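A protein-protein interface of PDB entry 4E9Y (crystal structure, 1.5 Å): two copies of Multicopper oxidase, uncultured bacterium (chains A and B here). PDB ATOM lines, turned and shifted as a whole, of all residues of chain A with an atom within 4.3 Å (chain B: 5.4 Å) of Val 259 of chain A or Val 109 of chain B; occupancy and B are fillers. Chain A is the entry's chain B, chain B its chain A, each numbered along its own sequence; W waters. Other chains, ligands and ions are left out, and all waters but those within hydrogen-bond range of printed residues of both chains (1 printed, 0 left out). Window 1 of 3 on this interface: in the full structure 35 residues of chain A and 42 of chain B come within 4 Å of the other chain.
Water W1 lies within hydrogen-bond range of N of Asn 108 of chain B (3.1 Å) and NE2 of His 265 of chain A (3.4 Å).
The side-chain amide oxygen (OD1) of Asn 110 of chain B is in hydrogen-bond range of a ring nitrogen (ND1) of His 265 of chain A, at 3.2 Å. OD2 of Asp 256 of chain A sits at hydrogen-bond distance from N of Gly 114 of chain B, at 3.2 Å.
Of the 11 printed residues of chain A, 4 touch a printed residue of chain B. Hydrophobic or aromatic side chains of chain B within 4 Å of the printed part of chain A: Val 109 and Val 113. Among the printed residues, 9 pairs touch across the chains.
Of chain B, only Val 109 (3.4 Å) comes within 4 Å of Val 259 of chain A. Printed residues of chain B within 4 Å of Thr 260 of chain A: Asn 110. Of the printed residues of chain A, Asn 108 of chain B touches His 265 (3.5 Å). Val 109 of chain B touches three residues of chain A.
O of Val 109 of chain B sits at hydrogen-bond distance from N of Gly 114 of chain B (3.1 Å). OG1 of Thr 260 of chain A is in hydrogen-bond range of O of Thr 257 of chain A. O of Val 259 of chain A is in hydrogen-bond range of ND1 of His 265 of chain A, 2.9 Å away. The backbone carbonyl oxygen (O) of Val 259 of chain A is in hydrogen-bond range of the backbone NH (N) of Gly 267 of chain A.
No position is printed for both chains. Of the 9 pairs that touch across the chains among the printed residues, none has its exchanged pair printed and touching as well.
OD2 of Asp 256 of chain A touches O of Val 109 of chain B, 3.8 Å away. Asp 256 of chain A touches Asn 110 of chain B. Asp 256 of chain A touches Val 113 of chain B (OD2 to C, 3.6 Å). Val 109 of chain B touches Val 259 of chain A. Thr 260 of chain A touches Asn 110 of chain B (CG2 to CG, 3.6 Å). His 265 of chain A touches Asn 108 of chain B (NE2 to N, 3.5 Å). His 265 of chain A touches Val 109 of chain B (CE1 to N, 3.6 Å).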
ATOM      1  N   ASP A 253     -23.958  -8.075 -29.679  1.00  0.00           N
ATOM      2  CA  ASP A 253     -25.210  -8.111 -30.444  1.00  0.00           C
ATOM      3  C   ASP A 253     -26.387  -7.969 -29.475  1.00  0.00           C
ATOM      4  O   ASP A 253     -26.470  -8.772 -28.550  1.00  0.00           O
ATOM      5  CB  ASP A 253     -25.296  -9.404 -31.228  1.00  0.00           C
ATOM      6  CG  ASP A 253     -26.445  -9.527 -32.200  1.00  0.00           C
ATOM      7  OD1 ASP A 253     -27.355  -8.657 -32.185  1.00  0.00           O
ATOM      8  OD2 ASP A 253     -26.390 -10.533 -32.956  1.00  0.00           O
ATOM      9  N   VAL A 255     -29.537  -8.212 -30.305  1.00  0.00           N
ATOM     10  CA  VAL A 255     -30.726  -9.018 -30.615  1.00  0.00           C
ATOM     11  C   VAL A 255     -30.871 -10.115 -29.555  1.00  0.00           C
ATOM     12  O   VAL A 255     -29.955 -10.941 -29.428  1.00  0.00           O
ATOM     13  CB  VAL A 255     -30.653  -9.651 -32.018  1.00  0.00           C
ATOM     14  CG1 VAL A 255     -31.816 -10.604 -32.257  1.00  0.00           C
ATOM     15  CG2 VAL A 255     -30.598  -8.554 -33.074  1.00  0.00           C
ATOM     16  N   ASP A 256     -31.968 -10.115 -28.814  1.00  0.00           N
ATOM     17  CA  ASP A 256     -32.141 -10.934 -27.611  1.00  0.00           C
ATOM     18  C   ASP A 256     -31.831 -12.397 -27.824  1.00  0.00           C
ATOM     19  O   ASP A 256     -31.086 -13.010 -27.036  1.00  0.00           O
ATOM     20  CB  ASP A 256     -33.577 -10.701 -27.094  1.00  0.00           C
ATOM     21  CG  ASP A 256     -33.703  -9.245 -26.631  1.00  0.00           C
ATOM     22  OD1 ASP A 256     -33.226  -8.294 -27.297  1.00  0.00           O
ATOM     23  OD2 ASP A 256     -34.299  -9.013 -25.556  1.00  0.00           O
ATOM     24  N   THR A 257     -32.346 -13.013 -28.874  1.00  0.00           N
ATOM     25  CA  THR A 257     -32.047 -14.434 -29.058  1.00  0.00           C
ATOM     26  C   THR A 257     -30.624 -14.743 -29.466  1.00  0.00           C
ATOM     27  O   THR A 257     -30.234 -15.918 -29.373  1.00  0.00           O
ATOM     28  CB  THR A 257     -32.990 -15.024 -30.145  1.00  0.00           C
ATOM     29  OG1 THR A 257     -32.839 -14.247 -31.338  1.00  0.00           O
ATOM     30  CG2 THR A 257     -34.431 -14.887 -29.702  1.00  0.00           C
ATOM     31  N   HIS A 258     -29.835 -13.782 -29.912  1.00  0.00           N
ATOM     32  CA  HIS A 258     -28.488 -14.018 -30.419  1.00  0.00           C
ATOM     33  C   HIS A 258     -27.463 -14.118 -29.302  1.00  0.00           C
ATOM     34  O   HIS A 258     -26.319 -14.514 -29.566  1.00  0.00           O
ATOM     35  CB  HIS A 258     -28.033 -12.879 -31.349  1.00  0.00           C
ATOM     36  CG  HIS A 258     -28.821 -12.874 -32.632  1.00  0.00           C
ATOM     37  ND1 HIS A 258     -28.520 -12.041 -33.680  1.00  0.00           N
ATOM     38  CD2 HIS A 258     -29.877 -13.630 -33.001  1.00  0.00           C
ATOM     39  CE1 HIS A 258     -29.371 -12.277 -34.671  1.00  0.00           C
ATOM     40  NE2 HIS A 258     -30.205 -13.231 -34.275  1.00  0.00           N
ATOM     41  N   VAL A 259     -27.861 -13.769 -28.079  1.00  0.00           N
ATOM     42  CA  VAL A 259     -26.855 -13.927 -27.010  1.00  0.00           C
ATOM     43  C   VAL A 259     -27.163 -15.226 -26.259  1.00  0.00           C
ATOM     44  O   VAL A 259     -27.168 -15.288 -25.033  1.00  0.00           O
ATOM     45  CB  VAL A 259     -26.743 -12.739 -26.054  1.00  0.00           C
ATOM     46  CG1 VAL A 259     -26.121 -11.557 -26.814  1.00  0.00           C
ATOM     47  CG2 VAL A 259     -28.069 -12.308 -25.460  1.00  0.00           C
ATOM     48  N   THR A 260     -27.434 -16.251 -27.035  1.00  0.00           N
ATOM     49  CA  THR A 260     -27.630 -17.615 -26.590  1.00  0.00           C
ATOM     50  C   THR A 260     -26.722 -18.547 -27.392  1.00  0.00           C
ATOM     51  O   THR A 260     -26.178 -18.130 -28.421  1.00  0.00           O
ATOM     52  CB  THR A 260     -29.079 -18.077 -26.750  1.00  0.00           C
ATOM     53  OG1 THR A 260     -29.445 -18.106 -28.143  1.00  0.00           O
ATOM     54  CG2 THR A 260     -29.959 -17.073 -26.010  1.00  0.00           C
ATOM     55  N   HIS A 265     -27.724 -19.443 -22.135  1.00  0.00           N
ATOM     56  CA  HIS A 265     -27.226 -18.072 -22.065  1.00  0.00           C
ATOM     57  C   HIS A 265     -26.149 -18.027 -20.983  1.00  0.00           C
ATOM     58  O   HIS A 265     -26.314 -18.782 -20.011  1.00  0.00           O
ATOM     59  CB  HIS A 265     -28.344 -17.079 -21.768  1.00  0.00           C
ATOM     60  CG  HIS A 265     -27.952 -15.680 -21.388  1.00  0.00           C
ATOM     61  ND1 HIS A 265     -28.001 -14.629 -22.284  1.00  0.00           N
ATOM     62  CD2 HIS A 265     -27.491 -15.118 -20.237  1.00  0.00           C
ATOM     63  CE1 HIS A 265     -27.598 -13.509 -21.701  1.00  0.00           C
ATOM     64  NE2 HIS A 265     -27.279 -13.775 -20.445  1.00  0.00           N
ATOM     65  N   PRO A 266     -25.120 -17.208 -21.111  1.00  0.00           N
ATOM     66  CA  PRO A 266     -24.869 -16.376 -22.291  1.00  0.00           C
ATOM     67  C   PRO A 266     -24.054 -17.099 -23.349  1.00  0.00           C
ATOM     68  O   PRO A 266     -23.434 -18.130 -23.131  1.00  0.00           O
ATOM     69  CB  PRO A 266     -24.006 -15.230 -21.738  1.00  0.00           C
ATOM     70  CG  PRO A 266     -23.175 -15.930 -20.700  1.00  0.00           C
ATOM     71  CD  PRO A 266     -24.064 -16.986 -20.105  1.00  0.00           C
ATOM     72  N   GLY A 267     -24.068 -16.481 -24.524  1.00  0.00           N
ATOM     73  CA  GLY A 267     -23.286 -16.984 -25.654  1.00  0.00           C
ATOM     74  C   GLY A 267     -23.384 -15.930 -26.753  1.00  0.00           C
ATOM     75  O   GLY A 267     -23.982 -14.867 -26.523  1.00  0.00           O
ATOM     76  N   ILE A 270     -20.338 -11.588 -28.401  1.00  0.00           N
ATOM     77  CA  ILE A 270     -20.059 -10.757 -27.252  1.00  0.00           C
ATOM     78  C   ILE A 270     -18.552 -10.640 -27.075  1.00  0.00           C
ATOM     79  O   ILE A 270     -17.841 -11.661 -27.115  1.00  0.00           O
ATOM     80  CB  ILE A 270     -20.640 -11.365 -25.953  1.00  0.00           C
ATOM     81  CG1 ILE A 270     -22.143 -11.665 -25.997  1.00  0.00           C
ATOM     82  CG2 ILE A 270     -20.250 -10.486 -24.751  1.00  0.00           C
ATOM     83  CD1 ILE A 270     -22.661 -12.369 -24.755  1.00  0.00           C
ATOM     84  N   HIS B 104     -32.529  -1.568 -18.558  1.00  0.00           N
ATOM     85  CA  HIS B 104     -33.069  -2.901 -18.647  1.00  0.00           C
ATOM     86  C   HIS B 104     -32.196  -3.872 -17.840  1.00  0.00           C
ATOM     87  O   HIS B 104     -31.027  -3.570 -17.582  1.00  0.00           O
ATOM     88  CB  HIS B 104     -33.199  -3.444 -20.076  1.00  0.00           C
ATOM     89  CG  HIS B 104     -31.938  -3.439 -20.894  1.00  0.00           C
ATOM     90  ND1 HIS B 104     -30.948  -4.392 -20.848  1.00  0.00           N
ATOM     91  CD2 HIS B 104     -31.524  -2.537 -21.822  1.00  0.00           C
ATOM     92  CE1 HIS B 104     -29.969  -4.075 -21.707  1.00  0.00           C
ATOM     93  NE2 HIS B 104     -30.307  -2.958 -22.305  1.00  0.00           N
ATOM     94  N   CYS B 105     -32.778  -5.005 -17.497  1.00  0.00           N
ATOM     95  CA  CYS B 105     -31.920  -5.953 -16.752  1.00  0.00           C
ATOM     96  C   CYS B 105     -30.822  -6.435 -17.674  1.00  0.00           C
ATOM     97  O   CYS B 105     -31.011  -6.443 -18.896  1.00  0.00           O
ATOM     98  CB  CYS B 105     -32.794  -7.101 -16.271  1.00  0.00           C
ATOM     99  SG  CYS B 105     -31.850  -8.372 -15.386  1.00  0.00           S
ATOM    100  N   HIS B 106     -29.682  -6.873 -17.158  1.00  0.00           N
ATOM    101  CA  HIS B 106     -28.639  -7.439 -17.999  1.00  0.00           C
ATOM    102  C   HIS B 106     -28.245  -8.855 -17.549  1.00  0.00           C
ATOM    103  O   HIS B 106     -27.142  -9.308 -17.876  1.00  0.00           O
ATOM    104  CB  HIS B 106     -27.392  -6.546 -18.002  1.00  0.00           C
ATOM    105  CG  HIS B 106     -26.772  -6.454 -19.363  1.00  0.00           C
ATOM    106  ND1 HIS B 106     -26.081  -7.509 -19.919  1.00  0.00           N
ATOM    107  CD2 HIS B 106     -26.743  -5.447 -20.266  1.00  0.00           C
ATOM    108  CE1 HIS B 106     -25.653  -7.152 -21.117  1.00  0.00           C
ATOM    109  NE2 HIS B 106     -26.034  -5.910 -21.351  1.00  0.00           N
ATOM    110  N   VAL B 107     -29.125  -9.537 -16.836  1.00  0.00           N
ATOM    111  CA  VAL B 107     -28.998 -10.934 -16.465  1.00  0.00           C
ATOM    112  C   VAL B 107     -29.966 -11.760 -17.338  1.00  0.00           C
ATOM    113  O   VAL B 107     -31.115 -11.310 -17.426  1.00  0.00           O
ATOM    114  CB  VAL B 107     -29.378 -11.184 -15.001  1.00  0.00           C
ATOM    115  CG1 VAL B 107     -29.262 -12.682 -14.696  1.00  0.00           C
ATOM    116  CG2 VAL B 107     -28.555 -10.384 -14.011  1.00  0.00           C
ATOM    117  N   ASN B 108     -29.541 -12.873 -17.903  1.00  0.00           N
ATOM    118  CA  ASN B 108     -30.450 -13.770 -18.626  1.00  0.00           C
ATOM    119  C   ASN B 108     -31.299 -12.978 -19.622  1.00  0.00           C
ATOM    120  O   ASN B 108     -32.520 -13.136 -19.741  1.00  0.00           O
ATOM    121  CB  ASN B 108     -31.323 -14.510 -17.613  1.00  0.00           C
ATOM    122  CG  ASN B 108     -30.689 -15.665 -16.852  1.00  0.00           C
ATOM    123  OD1 ASN B 108     -29.649 -16.230 -17.206  1.00  0.00           O
ATOM    124  ND2 ASN B 108     -31.311 -16.100 -15.746  1.00  0.00           N
ATOM    125  N   VAL B 109     -30.625 -12.054 -20.307  1.00  0.00           N
ATOM    126  CA  VAL B 109     -31.337 -11.039 -21.084  1.00  0.00           C
ATOM    127  C   VAL B 109     -32.267 -11.584 -22.158  1.00  0.00           C
ATOM    128  O   VAL B 109     -33.306 -10.952 -22.399  1.00  0.00           O
ATOM    129  CB  VAL B 109     -30.364 -10.025 -21.736  1.00  0.00           C
ATOM    130  CG1 VAL B 109     -29.454  -9.460 -20.656  1.00  0.00           C
ATOM    131  CG2 VAL B 109     -29.534 -10.611 -22.859  1.00  0.00           C
ATOM    132  N   ASN B 110     -31.931 -12.703 -22.801  1.00  0.00           N
ATOM    133  CA  ASN B 110     -32.793 -13.251 -23.840  1.00  0.00           C
ATOM    134  C   ASN B 110     -34.186 -13.461 -23.259  1.00  0.00           C
ATOM    135  O   ASN B 110     -35.179 -13.272 -23.951  1.00  0.00           O
ATOM    136  CB  ASN B 110     -32.280 -14.561 -24.445  1.00  0.00           C
ATOM    137  CG  ASN B 110     -31.947 -15.618 -23.410  1.00  0.00           C
ATOM    138  OD1 ASN B 110     -31.079 -15.395 -22.562  1.00  0.00           O
ATOM    139  ND2 ASN B 110     -32.611 -16.747 -23.417  1.00  0.00           N
ATOM    140  N   GLU B 111     -34.244 -13.841 -21.978  1.00  0.00           N
ATOM    141  CA  GLU B 111     -35.554 -14.058 -21.379  1.00  0.00           C
ATOM    142  C   GLU B 111     -36.038 -12.807 -20.660  1.00  0.00           C
ATOM    143  O   GLU B 111     -37.186 -12.389 -20.877  1.00  0.00           O
ATOM    144  CB  GLU B 111     -35.528 -15.225 -20.373  1.00  0.00           C
ATOM    145  CG  GLU B 111     -36.909 -15.570 -19.832  1.00  0.00           C
ATOM    146  CD  GLU B 111     -36.916 -16.363 -18.539  1.00  0.00           C
ATOM    147  OE1 GLU B 111     -35.869 -16.968 -18.216  1.00  0.00           O
ATOM    148  OE2 GLU B 111     -37.976 -16.373 -17.861  1.00  0.00           O
ATOM    149  N   HIS B 112     -35.181 -12.245 -19.800  1.00  0.00           N
ATOM    150  CA  HIS B 112     -35.663 -11.147 -18.944  1.00  0.00           C
ATOM    151  C   HIS B 112     -36.016  -9.909 -19.755  1.00  0.00           C
ATOM    152  O   HIS B 112     -37.018  -9.244 -19.476  1.00  0.00           O
ATOM    153  CB  HIS B 112     -34.626 -10.828 -17.863  1.00  0.00           C
ATOM    154  CG  HIS B 112     -34.523 -11.898 -16.815  1.00  0.00           C
ATOM    155  ND1 HIS B 112     -33.912 -11.648 -15.602  1.00  0.00           N
ATOM    156  CD2 HIS B 112     -34.938 -13.181 -16.799  1.00  0.00           C
ATOM    157  CE1 HIS B 112     -33.956 -12.750 -14.878  1.00  0.00           C
ATOM    158  NE2 HIS B 112     -34.567 -13.702 -15.573  1.00  0.00           N
ATOM    159  N   VAL B 113     -35.183  -9.594 -20.755  1.00  0.00           N
ATOM    160  CA  VAL B 113     -35.509  -8.413 -21.572  1.00  0.00           C
ATOM    161  C   VAL B 113     -36.418  -8.879 -22.685  1.00  0.00           C
ATOM    162  O   VAL B 113     -37.346  -8.179 -23.094  1.00  0.00           O
ATOM    163  CB  VAL B 113     -34.245  -7.724 -22.097  1.00  0.00           C
ATOM    164  CG1 VAL B 113     -34.601  -6.538 -22.985  1.00  0.00           C
ATOM    165  CG2 VAL B 113     -33.391  -7.271 -20.919  1.00  0.00           C
ATOM    166  N   GLY B 114     -36.213 -10.085 -23.190  1.00  0.00           N
ATOM    167  CA  GLY B 114     -37.007 -10.539 -24.331  1.00  0.00           C
ATOM    168  C   GLY B 114     -38.468 -10.750 -24.032  1.00  0.00           C
ATOM    169  O   GLY B 114     -39.315 -10.368 -24.866  1.00  0.00           O
HETATM  170  O   HOH W   1     -26.639 -13.476 -17.151  1.00  0.00           O
